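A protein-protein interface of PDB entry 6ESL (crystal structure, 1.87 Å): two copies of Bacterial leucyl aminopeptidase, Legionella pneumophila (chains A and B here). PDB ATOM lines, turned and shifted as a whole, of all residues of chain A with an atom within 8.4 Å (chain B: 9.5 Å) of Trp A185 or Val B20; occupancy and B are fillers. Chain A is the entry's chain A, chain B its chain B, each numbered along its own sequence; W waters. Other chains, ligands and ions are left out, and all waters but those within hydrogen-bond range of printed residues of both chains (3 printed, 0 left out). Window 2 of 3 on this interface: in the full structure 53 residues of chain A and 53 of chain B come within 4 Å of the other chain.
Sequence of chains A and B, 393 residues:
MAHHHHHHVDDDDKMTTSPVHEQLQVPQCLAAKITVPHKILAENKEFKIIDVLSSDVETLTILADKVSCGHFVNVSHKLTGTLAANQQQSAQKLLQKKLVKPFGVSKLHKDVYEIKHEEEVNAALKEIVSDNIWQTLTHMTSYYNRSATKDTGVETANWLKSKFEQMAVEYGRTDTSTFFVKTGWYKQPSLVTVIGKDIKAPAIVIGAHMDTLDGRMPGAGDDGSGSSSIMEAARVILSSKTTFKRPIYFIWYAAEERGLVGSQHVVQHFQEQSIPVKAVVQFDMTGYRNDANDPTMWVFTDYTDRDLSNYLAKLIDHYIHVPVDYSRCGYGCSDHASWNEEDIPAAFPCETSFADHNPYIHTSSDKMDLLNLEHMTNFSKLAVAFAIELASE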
ATOM      1  N   ALA A 148      25.814   9.568 -32.022  1.00  0.00           N
ATOM      2  CA  ALA A 148      24.607  10.204 -32.434  1.00  0.00           C
ATOM      3  C   ALA A 148      24.844  11.421 -33.347  1.00  0.00           C
ATOM      4  O   ALA A 148      23.918  11.860 -34.011  1.00  0.00           O
ATOM      5  CB  ALA A 148      23.790  10.587 -31.247  1.00  0.00           C
ATOM      6  N   THR A 149      26.091  11.915 -33.392  1.00  0.00           N
ATOM      7  CA  THR A 149      26.434  13.037 -34.234  1.00  0.00           C
ATOM      8  C   THR A 149      27.033  12.589 -35.576  1.00  0.00           C
ATOM      9  O   THR A 149      27.440  13.488 -36.318  1.00  0.00           O
ATOM     10  CB  THR A 149      27.454  13.992 -33.593  1.00  0.00           C
ATOM     11  OG1 THR A 149      28.644  13.254 -33.329  1.00  0.00           O
ATOM     12  CG2 THR A 149      26.885  14.681 -32.359  1.00  0.00           C
ATOM     13  N   LYS A 150      27.170  11.278 -35.814  1.00  0.00           N
ATOM     14  CA  LYS A 150      27.846  10.763 -36.982  1.00  0.00           C
ATOM     15  C   LYS A 150      27.009   9.936 -37.951  1.00  0.00           C
ATOM     16  O   LYS A 150      26.033   9.289 -37.553  1.00  0.00           O
ATOM     17  CB  LYS A 150      29.029   9.899 -36.572  1.00  0.00           C
ATOM     18  CG  LYS A 150      30.003  10.645 -35.677  1.00  0.00           C
ATOM     19  CD  LYS A 150      30.704  11.720 -36.476  1.00  0.00           C
ATOM     20  CE  LYS A 150      32.108  11.974 -35.971  1.00  0.00           C
ATOM     21  NZ  LYS A 150      32.005  12.849 -34.803  1.00  0.00           N
ATOM     22  N   LYS A 182      12.767  11.393 -33.759  1.00  0.00           N
ATOM     23  CA  LYS A 182      13.895  12.260 -33.942  1.00  0.00           C
ATOM     24  C   LYS A 182      14.571  12.794 -32.690  1.00  0.00           C
ATOM     25  O   LYS A 182      13.996  12.860 -31.663  1.00  0.00           O
ATOM     26  CB  LYS A 182      13.571  13.322 -34.991  1.00  0.00           C
ATOM     27  CG  LYS A 182      13.838  12.742 -36.369  1.00  0.00           C
ATOM     28  CD  LYS A 182      12.999  13.359 -37.454  1.00  0.00           C
ATOM     29  CE  LYS A 182      13.353  12.807 -38.819  1.00  0.00           C
ATOM     30  NZ  LYS A 182      12.851  13.726 -39.868  1.00  0.00           N
ATOM     31  N   THR A 183      15.813  13.170 -32.848  1.00  0.00           N
ATOM     32  CA  THR A 183      16.673  13.578 -31.774  1.00  0.00           C
ATOM     33  C   THR A 183      17.159  15.027 -31.830  1.00  0.00           C
ATOM     34  O   THR A 183      18.263  15.314 -31.531  1.00  0.00           O
ATOM     35  CB  THR A 183      17.893  12.622 -31.727  1.00  0.00           C
ATOM     36  OG1 THR A 183      17.506  11.302 -32.081  1.00  0.00           O
ATOM     37  CG2 THR A 183      18.503  12.609 -30.364  1.00  0.00           C
ATOM     38  N   GLY A 184      16.329  15.946 -32.276  1.00  0.00           N
ATOM     39  CA  GLY A 184      16.778  17.318 -32.391  1.00  0.00           C
ATOM     40  C   GLY A 184      17.924  17.492 -33.352  1.00  0.00           C
ATOM     41  O   GLY A 184      17.874  17.000 -34.433  1.00  0.00           O
ATOM     42  N   TRP A 185      18.976  18.163 -32.943  1.00  0.00           N
ATOM     43  CA  TRP A 185      20.094  18.413 -33.860  1.00  0.00           C
ATOM     44  C   TRP A 185      20.893  17.171 -34.001  1.00  0.00           C
ATOM     45  O   TRP A 185      21.718  17.108 -34.827  1.00  0.00           O
ATOM     46  CB  TRP A 185      21.005  19.662 -33.557  1.00  0.00           C
ATOM     47  CG  TRP A 185      21.727  19.522 -32.346  1.00  0.00           C
ATOM     48  CD1 TRP A 185      21.224  19.794 -31.101  1.00  0.00           C
ATOM     49  CD2 TRP A 185      23.077  19.035 -32.155  1.00  0.00           C
ATOM     50  NE1 TRP A 185      22.141  19.398 -30.122  1.00  0.00           N
ATOM     51  CE2 TRP A 185      23.301  18.997 -30.732  1.00  0.00           C
ATOM     52  CE3 TRP A 185      24.091  18.606 -33.011  1.00  0.00           C
ATOM     53  CZ2 TRP A 185      24.525  18.592 -30.158  1.00  0.00           C
ATOM     54  CZ3 TRP A 185      25.310  18.202 -32.438  1.00  0.00           C
ATOM     55  CH2 TRP A 185      25.506  18.191 -31.027  1.00  0.00           C
ATOM     56  N   TYR A 186      20.701  16.144 -33.135  1.00  0.00           N
ATOM     57  CA  TYR A 186      21.451  14.902 -33.364  1.00  0.00           C
ATOM     58  C   TYR A 186      20.873  14.176 -34.576  1.00  0.00           C
ATOM     59  O   TYR A 186      19.664  13.958 -34.664  1.00  0.00           O
ATOM     60  CB  TYR A 186      21.384  13.982 -32.140  1.00  0.00           C
ATOM     61  CG  TYR A 186      22.140  14.525 -30.959  1.00  0.00           C
ATOM     62  CD1 TYR A 186      23.550  14.367 -30.859  1.00  0.00           C
ATOM     63  CD2 TYR A 186      21.487  15.234 -29.969  1.00  0.00           C
ATOM     64  CE1 TYR A 186      24.265  14.878 -29.770  1.00  0.00           C
ATOM     65  CE2 TYR A 186      22.175  15.688 -28.813  1.00  0.00           C
ATOM     66  CZ  TYR A 186      23.573  15.518 -28.742  1.00  0.00           C
ATOM     67  OH  TYR A 186      24.217  16.051 -27.644  1.00  0.00           O
ATOM     68  N   LYS A 187      21.744  13.800 -35.484  1.00  0.00           N
ATOM     69  CA  LYS A 187      21.255  13.155 -36.715  1.00  0.00           C
ATOM     70  C   LYS A 187      20.806  11.704 -36.543  1.00  0.00           C
ATOM     71  O   LYS A 187      20.032  11.191 -37.305  1.00  0.00           O
ATOM     72  CB  LYS A 187      22.270  13.294 -37.821  1.00  0.00           C
ATOM     73  CG  LYS A 187      23.636  12.757 -37.505  1.00  0.00           C
ATOM     74  CD  LYS A 187      24.526  12.830 -38.761  1.00  0.00           C
ATOM     75  CE  LYS A 187      25.152  14.191 -38.954  1.00  0.00           C
ATOM     76  NZ  LYS A 187      26.364  13.921 -39.809  1.00  0.00           N
ATOM     77  N   GLN A 188      21.305  10.993 -35.529  1.00  0.00           N
ATOM     78  CA  GLN A 188      20.776   9.616 -35.242  1.00  0.00           C
ATOM     79  C   GLN A 188      19.393   9.703 -34.561  1.00  0.00           C
ATOM     80  O   GLN A 188      19.247  10.249 -33.436  1.00  0.00           O
ATOM     81  CB  GLN A 188      21.755   8.900 -34.336  1.00  0.00           C
ATOM     82  CG  GLN A 188      21.437   7.457 -33.885  1.00  0.00           C
ATOM     83  CD  GLN A 188      22.488   7.041 -32.876  1.00  0.00           C
ATOM     84  OE1 GLN A 188      22.454   7.537 -31.716  1.00  0.00           O
ATOM     85  NE2 GLN A 188      23.458   6.207 -33.297  1.00  0.00           N
ATOM     86  N   ARG A 258      25.033  10.921 -24.622  1.00  0.00           N
ATOM     87  CA  ARG A 258      25.006  12.366 -24.562  1.00  0.00           C
ATOM     88  C   ARG A 258      24.151  12.850 -23.438  1.00  0.00           C
ATOM     89  O   ARG A 258      23.915  14.012 -23.338  1.00  0.00           O
ATOM     90  CB  ARG A 258      24.475  12.957 -25.875  1.00  0.00           C
ATOM     91  CG  ARG A 258      25.172  12.510 -27.122  1.00  0.00           C
ATOM     92  CD  ARG A 258      26.569  13.068 -27.254  1.00  0.00           C
ATOM     93  NE  ARG A 258      26.609  14.511 -27.283  1.00  0.00           N
ATOM     94  CZ  ARG A 258      27.718  15.217 -27.348  1.00  0.00           C
ATOM     95  NH1 ARG A 258      28.872  14.629 -27.417  1.00  0.00           N
ATOM     96  NH2 ARG A 258      27.669  16.512 -27.376  1.00  0.00           N
ATOM     97  N   VAL A 261      19.483  11.685 -24.099  1.00  0.00           N
ATOM     98  CA  VAL A 261      18.757  12.402 -25.130  1.00  0.00           C
ATOM     99  C   VAL A 261      17.668  11.682 -25.891  1.00  0.00           C
ATOM    100  O   VAL A 261      16.577  12.100 -25.868  1.00  0.00           O
ATOM    101  CB  VAL A 261      19.701  13.064 -26.126  1.00  0.00           C
ATOM    102  CG1 VAL A 261      18.934  13.963 -27.093  1.00  0.00           C
ATOM    103  CG2 VAL A 261      20.743  13.859 -25.395  1.00  0.00           C
ATOM    104  N   HIS A 265      13.489  11.957 -25.632  1.00  0.00           N
ATOM    105  CA  HIS A 265      12.613  12.209 -26.863  1.00  0.00           C
ATOM    106  C   HIS A 265      11.509  11.139 -27.044  1.00  0.00           C
ATOM    107  O   HIS A 265      10.354  11.467 -27.255  1.00  0.00           O
ATOM    108  CB  HIS A 265      13.412  12.341 -28.146  1.00  0.00           C
ATOM    109  CG  HIS A 265      14.089  13.659 -28.311  1.00  0.00           C
ATOM    110  ND1 HIS A 265      13.549  14.703 -29.049  1.00  0.00           N
ATOM    111  CD2 HIS A 265      15.301  14.100 -27.871  1.00  0.00           C
ATOM    112  CE1 HIS A 265      14.396  15.723 -29.023  1.00  0.00           C
ATOM    113  NE2 HIS A 265      15.464  15.381 -28.328  1.00  0.00           N
ATOM    114  N   VAL B  20      27.407  24.418 -31.028  1.00  0.00           N
ATOM    115  CA  VAL B  20      26.181  24.641 -30.209  1.00  0.00           C
ATOM    116  C   VAL B  20      26.446  24.425 -28.731  1.00  0.00           C
ATOM    117  O   VAL B  20      27.464  23.847 -28.367  1.00  0.00           O
ATOM    118  CB  VAL B  20      24.929  23.797 -30.661  1.00  0.00           C
ATOM    119  CG1 VAL B  20      24.496  24.201 -32.049  1.00  0.00           C
ATOM    120  CG2 VAL B  20      25.118  22.304 -30.662  1.00  0.00           C
ATOM    121  N   HIS B  21      25.528  24.991 -27.929  1.00  0.00           N
ATOM    122  CA  HIS B  21      25.665  24.761 -26.525  1.00  0.00           C
ATOM    123  C   HIS B  21      24.592  23.774 -26.151  1.00  0.00           C
ATOM    124  O   HIS B  21      23.521  23.800 -26.702  1.00  0.00           O
ATOM    125  CB  HIS B  21      25.385  26.026 -25.644  1.00  0.00           C
ATOM    126  CG  HIS B  21      26.317  27.171 -25.850  1.00  0.00           C
ATOM    127  ND1 HIS B  21      26.064  28.461 -25.399  1.00  0.00           N
ATOM    128  CD2 HIS B  21      27.556  27.205 -26.394  1.00  0.00           C
ATOM    129  CE1 HIS B  21      27.094  29.236 -25.679  1.00  0.00           C
ATOM    130  NE2 HIS B  21      28.025  28.492 -26.249  1.00  0.00           N
ATOM    131  N   GLU B  22      24.779  23.128 -25.025  1.00  0.00           N
ATOM    132  CA  GLU B  22      23.853  22.204 -24.402  1.00  0.00           C
ATOM    133  C   GLU B  22      23.752  22.455 -22.912  1.00  0.00           C
ATOM    134  O   GLU B  22      24.651  22.999 -22.292  1.00  0.00           O
ATOM    135  CB  GLU B  22      24.250  20.735 -24.683  1.00  0.00           C
ATOM    136  CG  GLU B  22      24.494  20.412 -26.154  1.00  0.00           C
ATOM    137  CD  GLU B  22      24.651  18.927 -26.479  1.00  0.00           C
ATOM    138  OE1 GLU B  22      25.770  18.569 -26.823  1.00  0.00           O
ATOM    139  OE2 GLU B  22      23.651  18.221 -26.494  1.00  0.00           O
ATOM    140  N   GLN B  23      22.613  22.178 -22.376  1.00  0.00           N
ATOM    141  CA  GLN B  23      22.366  22.263 -20.985  1.00  0.00           C
ATOM    142  C   GLN B  23      22.258  20.859 -20.380  1.00  0.00           C
ATOM    143  O   GLN B  23      21.437  19.975 -20.806  1.00  0.00           O
ATOM    144  CB  GLN B  23      21.126  23.064 -20.677  1.00  0.00           C
ATOM    145  CG  GLN B  23      21.250  24.514 -21.298  1.00  0.00           C
ATOM    146  CD  GLN B  23      21.014  24.562 -22.826  1.00  0.00           C
ATOM    147  OE1 GLN B  23      20.028  23.945 -23.272  1.00  0.00           O
ATOM    148  NE2 GLN B  23      21.887  25.112 -23.549  1.00  0.00           N
ATOM    149  N   LEU B  24      23.038  20.723 -19.300  1.00  0.00           N
ATOM    150  CA  LEU B  24      23.141  19.439 -18.525  1.00  0.00           C
ATOM    151  C   LEU B  24      22.751  19.638 -17.100  1.00  0.00           C
ATOM    152  O   LEU B  24      23.195  20.649 -16.491  1.00  0.00           O
ATOM    153  CB  LEU B  24      24.561  18.972 -18.600  1.00  0.00           C
ATOM    154  CG  LEU B  24      25.176  18.878 -19.976  1.00  0.00           C
ATOM    155  CD1 LEU B  24      26.590  18.387 -19.889  1.00  0.00           C
ATOM    156  CD2 LEU B  24      24.305  17.968 -20.852  1.00  0.00           C
ATOM    157  N   ASP B  51      25.338  25.172 -18.561  1.00  0.00           N
ATOM    158  CA  ASP B  51      25.418  25.325 -19.983  1.00  0.00           C
ATOM    159  C   ASP B  51      26.842  25.091 -20.373  1.00  0.00           C
ATOM    160  O   ASP B  51      27.757  25.722 -19.783  1.00  0.00           O
ATOM    161  CB  ASP B  51      25.046  26.817 -20.358  1.00  0.00           C
ATOM    162  CG  ASP B  51      25.047  27.046 -21.834  1.00  0.00           C
ATOM    163  OD1 ASP B  51      26.106  27.310 -22.402  1.00  0.00           O
ATOM    164  OD2 ASP B  51      24.005  26.821 -22.461  1.00  0.00           O
ATOM    165  N   VAL B  52      27.053  24.350 -21.431  1.00  0.00           N
ATOM    166  CA  VAL B  52      28.383  24.085 -21.913  1.00  0.00           C
ATOM    167  C   VAL B  52      28.386  23.962 -23.406  1.00  0.00           C
ATOM    168  O   VAL B  52      27.369  23.803 -23.987  1.00  0.00           O
ATOM    169  CB  VAL B  52      28.902  22.750 -21.369  1.00  0.00           C
ATOM    170  CG1 VAL B  52      28.931  22.787 -19.872  1.00  0.00           C
ATOM    171  CG2 VAL B  52      28.031  21.607 -21.851  1.00  0.00           C
ATOM    172  N   LEU B  53      29.536  24.067 -24.028  1.00  0.00           N
ATOM    173  CA  LEU B  53      29.632  23.835 -25.449  1.00  0.00           C
ATOM    174  C   LEU B  53      29.409  22.350 -25.706  1.00  0.00           C
ATOM    175  O   LEU B  53      29.840  21.535 -24.928  1.00  0.00           O
ATOM    176  CB  LEU B  53      31.016  24.125 -25.946  1.00  0.00           C
ATOM    177  CG  LEU B  53      31.562  25.536 -26.058  1.00  0.00           C
ATOM    178  CD1 LEU B  53      32.786  25.449 -26.922  1.00  0.00           C
ATOM    179  CD2 LEU B  53      30.532  26.433 -26.682  1.00  0.00           C
ATOM    180  N   SER B  54      28.818  21.981 -26.834  1.00  0.00           N
ATOM    181  CA  SER B  54      28.604  20.572 -27.180  1.00  0.00           C
ATOM    182  C   SER B  54      29.884  19.786 -27.387  1.00  0.00           C
ATOM    183  O   SER B  54      29.928  18.603 -27.189  1.00  0.00           O
ATOM    184  CB  SER B  54      27.673  20.381 -28.366  1.00  0.00           C
ATOM    185  OG  SER B  54      28.245  20.878 -29.521  1.00  0.00           O
ATOM    186  N   SER B  55      30.909  20.464 -27.836  1.00  0.00           N
ATOM    187  CA  SER B  55      32.201  19.900 -28.032  1.00  0.00           C
ATOM    188  C   SER B  55      32.869  19.467 -26.720  1.00  0.00           C
ATOM    189  O   SER B  55      33.862  18.841 -26.759  1.00  0.00           O
ATOM    190  CB  SER B  55      33.082  20.920 -28.749  1.00  0.00           C
ATOM    191  OG  SER B  55      33.249  22.048 -27.970  1.00  0.00           O
ATOM    192  N   ASP B  56      32.364  19.887 -25.580  1.00  0.00           N
ATOM    193  CA  ASP B  56      32.924  19.544 -24.268  1.00  0.00           C
ATOM    194  C   ASP B  56      32.135  18.460 -23.536  1.00  0.00           C
ATOM    195  O   ASP B  56      32.558  18.071 -22.438  1.00  0.00           O
ATOM    196  CB  ASP B  56      33.023  20.830 -23.369  1.00  0.00           C
ATOM    197  CG  ASP B  56      34.048  21.779 -23.805  1.00  0.00           C
ATOM    198  OD1 ASP B  56      35.074  21.420 -24.393  1.00  0.00           O
ATOM    199  OD2 ASP B  56      33.880  23.011 -23.573  1.00  0.00           O
ATOM    200  N   VAL B  57      31.012  17.983 -24.082  1.00  0.00           N
ATOM    201  CA  VAL B  57      30.152  17.035 -23.402  1.00  0.00           C
ATOM    202  C   VAL B  57      30.850  15.714 -23.150  1.00  0.00           C
ATOM    203  O   VAL B  57      30.676  15.142 -22.105  1.00  0.00           O
ATOM    204  CB  VAL B  57      28.803  16.848 -24.145  1.00  0.00           C
ATOM    205  CG1 VAL B  57      28.006  15.703 -23.666  1.00  0.00           C
ATOM    206  CG2 VAL B  57      27.964  18.139 -24.056  1.00  0.00           C
ATOM    207  N   ASN B  74      20.943  15.330 -20.091  1.00  0.00           N
ATOM    208  CA  ASN B  74      20.857  16.411 -21.083  1.00  0.00           C
ATOM    209  C   ASN B  74      19.469  16.998 -21.039  1.00  0.00           C
ATOM    210  O   ASN B  74      18.486  16.321 -21.305  1.00  0.00           O
ATOM    211  CB  ASN B  74      21.204  15.892 -22.473  1.00  0.00           C
ATOM    212  CG  ASN B  74      21.575  16.964 -23.421  1.00  0.00           C
ATOM    213  OD1 ASN B  74      20.857  17.957 -23.455  1.00  0.00           O
ATOM    214  ND2 ASN B  74      22.680  16.860 -24.134  1.00  0.00           N
ATOM    215  N   SER B  76      18.628  20.012 -22.566  1.00  0.00           N
ATOM    216  CA  SER B  76      18.501  21.000 -23.599  1.00  0.00           C
ATOM    217  C   SER B  76      17.107  20.992 -24.241  1.00  0.00           C
ATOM    218  O   SER B  76      16.515  22.081 -24.483  1.00  0.00           O
ATOM    219  CB  SER B  76      19.494  20.773 -24.693  1.00  0.00           C
ATOM    220  OG  SER B  76      20.831  20.647 -24.270  1.00  0.00           O
ATOM    221  N   HIS B  77      16.582  19.795 -24.517  1.00  0.00           N
ATOM    222  CA  HIS B  77      15.262  19.675 -25.150  1.00  0.00           C
ATOM    223  C   HIS B  77      14.200  20.392 -24.310  1.00  0.00           C
ATOM    224  O   HIS B  77      13.309  21.021 -24.842  1.00  0.00           O
ATOM    225  CB  HIS B  77      14.852  18.196 -25.442  1.00  0.00           C
ATOM    226  CG  HIS B  77      13.577  18.056 -26.253  1.00  0.00           C
ATOM    227  ND1 HIS B  77      13.309  18.807 -27.394  1.00  0.00           N
ATOM    228  CD2 HIS B  77      12.496  17.245 -26.089  1.00  0.00           C
ATOM    229  CE1 HIS B  77      12.125  18.480 -27.885  1.00  0.00           C
ATOM    230  NE2 HIS B  77      11.611  17.534 -27.113  1.00  0.00           N
HETATM  231  O   HOH W   1      21.326  19.222 -27.345  1.00  0.00           O
HETATM  232  O   HOH W   2      31.370  16.252 -26.908  1.00  0.00           O
HETATM  233  O   HOH W   3      21.499  21.916 -27.913  1.00  0.00           O
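OH of Tyr A186 lies within hydrogen-bond range of OE2 of Glu B22 (2.5 Å).
The side-chain carboxylate (OE1) of Glu B22 is in salt-bridge range of the guanidinium group (NH2) of Arg A258.
The backbone carbonyl oxygen of Ser B54 sits at hydrogen-bond distance from the guanidinium group of Arg A258, at 3.1 Å.
The side-chain amide nitrogen (ND2) of Asn B74 lies within hydrogen-bond range of the backbone carbonyl oxygen (O) of Arg A258, at 3.2 Å.
The backbone carbonyl oxygen (O) of Lys A182 sits at hydrogen-bond distance from a ring nitrogen (ND1) of His A265 (3.2 Å).
O of Val B20 sits at hydrogen-bond distance from N of Ser B54, 2.8 Å away.
The backbone NH (N) of Glu B22 lies within hydrogen-bond range of the backbone carbonyl oxygen (O) of Val B52, at 2.9 Å.
ND2 of Asn B74 is in hydrogen-bond range of OE2 of Glu B22 (2.9 Å).
The side-chain amide oxygen of Asn B74 sits close to the backbone carbonyl oxygen of Gln B23, 3.4 Å away.
The side-chain hydroxyl (OG) of Ser B76 lies within hydrogen-bond range of the side-chain amide oxygen (OD1) of Asn B74 (2.8 Å).
CG2 of Val B20 touches CE2 of Trp A185, 3.8 Å away.
Glu B22 touches Trp A185.
OH of Tyr A186 touches ND2 of Asn B74 (3.9 Å).
Val B57 touches Arg A258 (CB to NH2, 3.4 Å).
Val A261 touches Asn B74.
His A265 touches His B77.
Trp A185 touches just these residues of chain B: Val B20 and Glu B22.
Val B20 touches just one residue of chain A: Trp A185.
No residue of chain B comes within 4 Å of Gly A184.
Of chain B, only Glu B22 and Asn B74 come within 4 Å of Tyr A186.
Printed residues of chain B within 4 Å of Val A261: Asn B74.
Printed residues of chain A within 4 Å of Asn B74: Tyr A186 (3.9 Å), Arg A258 (3.2 Å) and Val A261 (3.6 Å).
Thr A149 touches none of the printed residues of chain B.
Lys A150 touches none of the printed residues of chain B.
The nearest residue of chain B that does not touch Trp A185 is Ser B54 (4.04 Å).
The nearest printed residue of chain B that does not touch Val A261 is Glu B22 (5.4 Å).
Of the 15 printed residues of chain B, 6 touch a printed residue of chain A.
Hydrophobic or aromatic side chains of chain B that line the printed part of chain A: Val B20, Val B57 and His B77.
Along chain B the printed residues that touch a printed residue of chain A span positions 20 to 77.
Of the 13 printed residues of chain A, 5 touch a printed residue of chain B.
Hydrophobic or aromatic side chains of chain A within 4 Å of the printed part of chain B: Trp A185, Tyr A186, Val A261 and His A265.
Along chain A the printed residues that touch a printed residue of chain B span positions 185 to 265.
No position is printed for both chains.
Of the 10 pairs that touch across the chains among the printed residues, none has its exchanged pair printed and touching as well.
Water W1 lies within hydrogen-bond range of the side-chain carboxylate (OE2) of Glu B22 (2.7 Å), the indole nitrogen (NE1) of Trp A185 (2.9 Å) and the side-chain hydroxyl (OG) of Ser B76 (3.4 Å).
Water W2 lies within hydrogen-bond range of O of Ser B54 (2.8 Å), NH1 of Arg A258 (3.0 Å) and N of Val B57 (3.3 Å).
Water W3 bridges O of His B21 and NE1 of Trp A185.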
